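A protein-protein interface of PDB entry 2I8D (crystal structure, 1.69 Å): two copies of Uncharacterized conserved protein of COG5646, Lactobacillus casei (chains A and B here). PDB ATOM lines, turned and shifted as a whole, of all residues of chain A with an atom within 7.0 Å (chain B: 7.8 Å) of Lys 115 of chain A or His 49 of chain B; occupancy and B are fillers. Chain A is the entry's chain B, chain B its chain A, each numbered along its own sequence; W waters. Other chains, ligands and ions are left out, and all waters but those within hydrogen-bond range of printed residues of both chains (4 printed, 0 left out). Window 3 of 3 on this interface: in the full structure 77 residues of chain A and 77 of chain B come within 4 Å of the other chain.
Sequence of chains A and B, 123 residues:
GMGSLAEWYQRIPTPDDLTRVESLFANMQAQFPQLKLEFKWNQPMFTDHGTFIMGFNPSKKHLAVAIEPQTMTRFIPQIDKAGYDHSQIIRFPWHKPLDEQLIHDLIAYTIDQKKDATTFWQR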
ATOM      1  N   THR A 110      20.989   7.526  19.307  1.00  0.00           N
ATOM      2  CA  THR A 110      19.921   6.564  19.163  1.00  0.00           C
ATOM      3  C   THR A 110      19.395   6.575  17.717  1.00  0.00           C
ATOM      4  O   THR A 110      19.150   5.518  17.141  1.00  0.00           O
ATOM      5  CB  THR A 110      18.804   6.826  20.209  1.00  0.00           C
ATOM      6  OG1 THR A 110      19.386   6.791  21.525  1.00  0.00           O
ATOM      7  CG2 THR A 110      17.729   5.701  20.117  1.00  0.00           C
ATOM      8  N   ILE A 111      19.240   7.779  17.141  1.00  0.00           N
ATOM      9  CA  ILE A 111      18.808   7.914  15.763  1.00  0.00           C
ATOM     10  C   ILE A 111      19.749   7.138  14.831  1.00  0.00           C
ATOM     11  O   ILE A 111      19.312   6.357  13.979  1.00  0.00           O
ATOM     12  CB  ILE A 111      18.732   9.392  15.346  1.00  0.00           C
ATOM     13  CG1 ILE A 111      17.482  10.029  15.977  1.00  0.00           C
ATOM     14  CG2 ILE A 111      18.659   9.579  13.831  1.00  0.00           C
ATOM     15  CD1 ILE A 111      17.383  11.536  15.735  1.00  0.00           C
ATOM     16  N   ASP A 112      21.044   7.378  14.994  1.00  0.00           N
ATOM     17  CA  ASP A 112      22.033   6.707  14.151  1.00  0.00           C
ATOM     18  C   ASP A 112      21.901   5.192  14.329  1.00  0.00           C
ATOM     19  O   ASP A 112      21.898   4.429  13.351  1.00  0.00           O
ATOM     20  CB  ASP A 112      23.426   7.166  14.503  1.00  0.00           C
ATOM     21  CG  ASP A 112      24.491   6.423  13.686  1.00  0.00           C
ATOM     22  OD1 ASP A 112      24.684   6.721  12.480  1.00  0.00           O
ATOM     23  OD2 ASP A 112      25.064   5.504  14.260  1.00  0.00           O
ATOM     24  N   GLN A 113      21.827   4.724  15.573  1.00  0.00           N
ATOM     25  CA  GLN A 113      21.696   3.301  15.817  1.00  0.00           C
ATOM     26  C   GLN A 113      20.408   2.684  15.253  1.00  0.00           C
ATOM     27  O   GLN A 113      20.417   1.502  14.886  1.00  0.00           O
ATOM     28  CB  GLN A 113      21.867   2.949  17.295  1.00  0.00           C
ATOM     29  CG  GLN A 113      23.258   3.282  17.870  1.00  0.00           C
ATOM     30  CD  GLN A 113      24.409   2.453  17.276  1.00  0.00           C
ATOM     31  OE1 GLN A 113      24.292   1.248  17.140  1.00  0.00           O
ATOM     32  NE2 GLN A 113      25.514   3.113  16.927  1.00  0.00           N
ATOM     33  N   LYS A 114      19.324   3.449  15.171  1.00  0.00           N
ATOM     34  CA  LYS A 114      18.045   2.933  14.686  1.00  0.00           C
ATOM     35  C   LYS A 114      17.802   3.124  13.184  1.00  0.00           C
ATOM     36  O   LYS A 114      16.727   2.733  12.670  1.00  0.00           O
ATOM     37  CB  LYS A 114      16.922   3.552  15.469  1.00  0.00           C
ATOM     38  CG  LYS A 114      16.989   3.211  16.948  1.00  0.00           C
ATOM     39  CD  LYS A 114      16.149   2.033  17.303  1.00  0.00           C
ATOM     40  CE  LYS A 114      15.958   1.947  18.813  1.00  0.00           C
ATOM     41  NZ  LYS A 114      14.491   1.915  19.145  1.00  0.00           N
ATOM     42  N   LYS A 115      18.802   3.625  12.462  1.00  0.00           N
ATOM     43  CA  LYS A 115      18.629   3.959  11.056  1.00  0.00           C
ATOM     44  C   LYS A 115      17.993   2.816  10.265  1.00  0.00           C
ATOM     45  O   LYS A 115      17.112   3.045   9.446  1.00  0.00           O
ATOM     46  CB  LYS A 115      19.972   4.347  10.424  1.00  0.00           C
ATOM     47  CG  LYS A 115      19.825   5.011   9.058  1.00  0.00           C
ATOM     48  CD  LYS A 115      21.139   5.007   8.276  1.00  0.00           C
ATOM     49  N   ASP A 116      18.454   1.587  10.494  1.00  0.00           N
ATOM     50  CA  ASP A 116      17.964   0.433   9.732  1.00  0.00           C
ATOM     51  C   ASP A 116      17.087  -0.490  10.575  1.00  0.00           C
ATOM     52  O   ASP A 116      16.865  -1.646  10.217  1.00  0.00           O
ATOM     53  CB  ASP A 116      19.160  -0.356   9.167  1.00  0.00           C
ATOM     54  CG  ASP A 116      20.059   0.485   8.270  1.00  0.00           C
ATOM     55  OD1 ASP A 116      19.561   1.275   7.452  1.00  0.00           O
ATOM     56  OD2 ASP A 116      21.303   0.343   8.368  1.00  0.00           O
ATOM     57  N   ALA A 117      16.576   0.004  11.697  1.00  0.00           N
ATOM     58  CA  ALA A 117      15.779  -0.816  12.613  1.00  0.00           C
ATOM     59  C   ALA A 117      14.435  -1.209  12.012  1.00  0.00           C
ATOM     60  O   ALA A 117      13.799  -0.399  11.312  1.00  0.00           O
ATOM     61  CB  ALA A 117      15.524  -0.049  13.943  1.00  0.00           C
ATOM     62  N   THR A 118      13.990  -2.431  12.341  1.00  0.00           N
ATOM     63  CA  THR A 118      12.734  -3.000  11.822  1.00  0.00           C
ATOM     64  C   THR A 118      11.689  -3.290  12.898  1.00  0.00           C
ATOM     65  O   THR A 118      10.652  -3.873  12.596  1.00  0.00           O
ATOM     66  CB  THR A 118      12.979  -4.292  11.038  1.00  0.00           C
ATOM     67  OG1 THR A 118      13.519  -5.287  11.916  1.00  0.00           O
ATOM     68  CG2 THR A 118      13.910  -4.021   9.842  1.00  0.00           C
ATOM     69  N   THR A 119      11.975  -2.894  14.144  1.00  0.00           N
ATOM     70  CA  THR A 119      11.028  -2.981  15.243  1.00  0.00           C
ATOM     71  C   THR A 119      10.967  -1.642  15.953  1.00  0.00           C
ATOM     72  O   THR A 119      11.901  -0.821  15.859  1.00  0.00           O
ATOM     73  CB  THR A 119      11.453  -4.081  16.284  1.00  0.00           C
ATOM     74  OG1 THR A 119      12.759  -3.781  16.809  1.00  0.00           O
ATOM     75  CG2 THR A 119      11.505  -5.463  15.645  1.00  0.00           C
ATOM     76  N   GLN B  34      13.006  15.428  11.902  1.00  0.00           N
ATOM     77  CA  GLN B  34      12.369  14.178  11.512  1.00  0.00           C
ATOM     78  C   GLN B  34      11.597  13.495  12.652  1.00  0.00           C
ATOM     79  O   GLN B  34      10.705  12.666  12.409  1.00  0.00           O
ATOM     80  CB  GLN B  34      13.426  13.204  10.972  1.00  0.00           C
ATOM     81  CG  GLN B  34      14.408  12.665  12.036  1.00  0.00           C
ATOM     82  CD  GLN B  34      15.711  13.437  12.145  1.00  0.00           C
ATOM     83  OE1 GLN B  34      15.715  14.627  12.389  1.00  0.00           O
ATOM     84  NE2 GLN B  34      16.847  12.724  12.000  1.00  0.00           N
ATOM     85  N   LEU B  35      11.937  13.840  13.896  1.00  0.00           N
ATOM     86  CA  LEU B  35      11.314  13.195  15.048  1.00  0.00           C
ATOM     87  C   LEU B  35       9.842  13.526  15.147  1.00  0.00           C
ATOM     88  O   LEU B  35       9.432  14.653  14.874  1.00  0.00           O
ATOM     89  CB  LEU B  35      11.977  13.638  16.334  1.00  0.00           C
ATOM     90  CG  LEU B  35      13.395  13.207  16.653  1.00  0.00           C
ATOM     91  CD1 LEU B  35      13.810  13.786  18.023  1.00  0.00           C
ATOM     92  CD2 LEU B  35      13.511  11.698  16.627  1.00  0.00           C
ATOM     93  N   LYS B  36       9.057  12.529  15.523  1.00  0.00           N
ATOM     94  CA  LYS B  36       7.652  12.664  15.778  1.00  0.00           C
ATOM     95  C   LYS B  36       7.437  12.582  17.282  1.00  0.00           C
ATOM     96  O   LYS B  36       7.945  11.680  17.932  1.00  0.00           O
ATOM     97  CB  LYS B  36       6.916  11.542  15.061  1.00  0.00           C
ATOM     98  CG  LYS B  36       5.454  11.559  15.046  1.00  0.00           C
ATOM     99  CD  LYS B  36       4.963  10.441  14.092  1.00  0.00           C
ATOM    100  CE  LYS B  36       3.476  10.144  14.275  1.00  0.00           C
ATOM    101  NZ  LYS B  36       2.893   9.401  13.111  1.00  0.00           N
ATOM    102  N   GLU B  38       4.975  11.587  19.828  1.00  0.00           N
ATOM    103  CA  GLU B  38       3.787  10.783  19.928  1.00  0.00           C
ATOM    104  C   GLU B  38       3.405  10.659  21.380  1.00  0.00           C
ATOM    105  O   GLU B  38       4.217  10.877  22.269  1.00  0.00           O
ATOM    106  CB  GLU B  38       4.041   9.388  19.370  1.00  0.00           C
ATOM    107  CG  GLU B  38       4.465   9.384  17.907  1.00  0.00           C
ATOM    108  CD  GLU B  38       4.318   8.032  17.231  1.00  0.00           C
ATOM    109  OE1 GLU B  38       3.267   7.391  17.383  1.00  0.00           O
ATOM    110  OE2 GLU B  38       5.234   7.615  16.507  1.00  0.00           O
ATOM    111  N   THR B  47       9.698   9.485  18.377  1.00  0.00           N
ATOM    112  CA  THR B  47       9.885   8.351  17.500  1.00  0.00           C
ATOM    113  C   THR B  47      10.476   8.832  16.145  1.00  0.00           C
ATOM    114  O   THR B  47      10.363   9.991  15.765  1.00  0.00           O
ATOM    115  CB  THR B  47       8.586   7.573  17.284  1.00  0.00           C
ATOM    116  OG1 THR B  47       7.713   8.329  16.432  1.00  0.00           O
ATOM    117  CG2 THR B  47       7.908   7.251  18.635  1.00  0.00           C
ATOM    118  N   ASP B  48      11.168   7.932  15.455  1.00  0.00           N
ATOM    119  CA  ASP B  48      11.770   8.225  14.170  1.00  0.00           C
ATOM    120  C   ASP B  48      11.497   7.038  13.240  1.00  0.00           C
ATOM    121  O   ASP B  48      11.831   5.896  13.580  1.00  0.00           O
ATOM    122  CB  ASP B  48      13.289   8.432  14.344  1.00  0.00           C
ATOM    123  CG  ASP B  48      13.991   8.993  13.099  1.00  0.00           C
ATOM    124  OD1 ASP B  48      13.352   9.612  12.235  1.00  0.00           O
ATOM    125  OD2 ASP B  48      15.221   8.801  13.001  1.00  0.00           O
ATOM    126  N   HIS B  49      10.842   7.317  12.103  1.00  0.00           N
ATOM    127  CA  HIS B  49      10.433   6.260  11.159  1.00  0.00           C
ATOM    128  C   HIS B  49       9.914   4.972  11.872  1.00  0.00           C
ATOM    129  O   HIS B  49      10.328   3.875  11.558  1.00  0.00           O
ATOM    130  CB  HIS B  49      11.546   5.972  10.154  1.00  0.00           C
ATOM    131  CG  HIS B  49      12.834   5.539  10.776  1.00  0.00           C
ATOM    132  ND1 HIS B  49      13.068   4.235  11.169  1.00  0.00           N
ATOM    133  CD2 HIS B  49      13.971   6.224  11.033  1.00  0.00           C
ATOM    134  CE1 HIS B  49      14.277   4.151  11.687  1.00  0.00           C
ATOM    135  NE2 HIS B  49      14.842   5.344  11.620  1.00  0.00           N
ATOM    136  N   GLY B  50       8.991   5.161  12.833  1.00  0.00           N
ATOM    137  CA  GLY B  50       8.308   4.056  13.501  1.00  0.00           C
ATOM    138  C   GLY B  50       9.135   3.316  14.553  1.00  0.00           C
ATOM    139  O   GLY B  50       8.844   2.153  14.879  1.00  0.00           O
ATOM    140  N   THR B  51      10.183   3.977  15.046  1.00  0.00           N
ATOM    141  CA  THR B  51      11.083   3.418  16.069  1.00  0.00           C
ATOM    142  C   THR B  51      11.210   4.361  17.259  1.00  0.00           C
ATOM    143  O   THR B  51      11.130   5.576  17.114  1.00  0.00           O
ATOM    144  CB  THR B  51      12.493   3.054  15.514  1.00  0.00           C
ATOM    145  OG1 THR B  51      13.286   4.244  15.358  1.00  0.00           O
ATOM    146  CG2 THR B  51      12.394   2.273  14.191  1.00  0.00           C
ATOM    147  N   PHE B  52      11.323   3.774  18.449  1.00  0.00           N
ATOM    148  CA  PHE B  52      11.481   4.539  19.670  1.00  0.00           C
ATOM    149  C   PHE B  52      12.808   5.238  19.760  1.00  0.00           C
ATOM    150  O   PHE B  52      13.859   4.611  19.555  1.00  0.00           O
ATOM    151  CB  PHE B  52      11.345   3.590  20.862  1.00  0.00           C
ATOM    152  CG  PHE B  52      11.566   4.238  22.178  1.00  0.00           C
ATOM    153  CD1 PHE B  52      10.563   4.941  22.826  1.00  0.00           C
ATOM    154  CD2 PHE B  52      12.817   4.171  22.784  1.00  0.00           C
ATOM    155  CE1 PHE B  52      10.802   5.506  24.038  1.00  0.00           C
ATOM    156  CE2 PHE B  52      13.054   4.734  24.012  1.00  0.00           C
ATOM    157  CZ  PHE B  52      12.044   5.387  24.657  1.00  0.00           C
ATOM    158  N   ILE B  53      12.763   6.523  20.099  1.00  0.00           N
ATOM    159  CA  ILE B  53      13.990   7.262  20.382  1.00  0.00           C
ATOM    160  C   ILE B  53      14.141   7.644  21.869  1.00  0.00           C
ATOM    161  O   ILE B  53      15.184   7.424  22.464  1.00  0.00           O
ATOM    162  CB  ILE B  53      14.124   8.515  19.471  1.00  0.00           C
ATOM    163  CG1 ILE B  53      14.108   8.137  17.983  1.00  0.00           C
ATOM    164  CG2 ILE B  53      15.366   9.319  19.814  1.00  0.00           C
ATOM    165  CD1 ILE B  53      15.222   7.170  17.547  1.00  0.00           C
HETATM  166  O   HOH W   1      12.430   1.720  10.465  1.00  0.00           O
HETATM  167  O   HOH W   2      17.363   6.016  23.505  1.00  0.00           O
HETATM  168  O   HOH W   3      15.882   5.140   8.369  1.00  0.00           O
HETATM  169  O   HOH W   4      16.996   6.528  12.668  1.00  0.00           O
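Of the printed residues of chain B, Lys 115 of chain A touches His 49.
His 49 of chain B touches just these residues of chain A: Lys 114 and Lys 115.
Of the printed residues of chain A, Gln 34 of chain B touches Ile 111 (3.96 Å).
Printed residues of chain A within 4 Å of Phe 52 of chain B: Lys 114.
Of the printed residues of chain B, Ile 111 of chain A touches Gln 34, Leu 35, Asp 48 and Ile 53.
Printed residues of chain A within 4 Å of Thr 51 of chain B: Lys 114, Ala 117 and Thr 119.
Thr 118 of chain A touches none of the printed residues of chain B.
Among the printed residues, merely in contact across the chains: Thr 110 of chain A with Ile 53 of chain B (3.9 Å), Ile 111 of chain A with Gln 34 of chain B (3.96 Å), Ile 111 of chain A with Leu 35 of chain B (3.98 Å), Ile 111 of chain A with Asp 48 of chain B (3.6 Å), Ile 111 of chain A with Ile 53 of chain B (3.97 Å), Lys 114 of chain A with Thr 51 of chain B (3.7 Å), Lys 115 of chain A with His 49 of chain B (3.8 Å), Ala 117 of chain A with Thr 51 of chain B (3.9 Å) and Thr 119 of chain A with Thr 51 of chain B (3.5 Å).
The backbone carbonyl oxygen (O) of Asp 48 of chain B sits at hydrogen-bond distance from the side-chain hydroxyl (OG1) of Thr 51 of chain B (2.8 Å).
No position is printed for both chains.
Of the 11 pairs that touch across the chains among the printed residues, none has its exchanged pair printed and touching as well.
Hydrophobic or aromatic side chains of chain B that line the printed part of chain A: Leu 35, His 49, Phe 52 and Ile 53.
Among the printed residues, no Asp or Glu carboxylate lies within 4 Å of a Lys or Arg side-chain nitrogen of the other chain.
A ring nitrogen (NE2) of His 49 of chain B lies close to the backbone carbonyl oxygen (O) of Lys 114 of chain A.
The backbone carbonyl oxygen (O) of Phe 52 of chain B is in hydrogen-bond range of the side-chain amino group (NZ) of Lys 114 of chain A, at 2.8 Å.
Water W3 bridges the backbone carbonyl oxygen of Lys 115 of chain A (2.7 Å) and a ring nitrogen (NE2) of His 49 of chain B (3.4 Å).
Water W1 lies within hydrogen-bond range of O of Ala 117 of chain A (2.7 Å) and ND1 of His 49 of chain B (2.7 Å).
Water W4 lies within hydrogen-bond range of the backbone carbonyl oxygen (O) of Ile 111 of chain A, a ring nitrogen (NE2) of His 49 of chain B, the side-chain carboxylate (OD2) of Asp 48 of chain B and the backbone NH (N) of Lys 115 of chain A.
Water W2 bridges the backbone carbonyl oxygen of Ile 53 of chain B (2.8 Å) and the side-chain hydroxyl of Thr 110 of chain A (2.9 Å).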
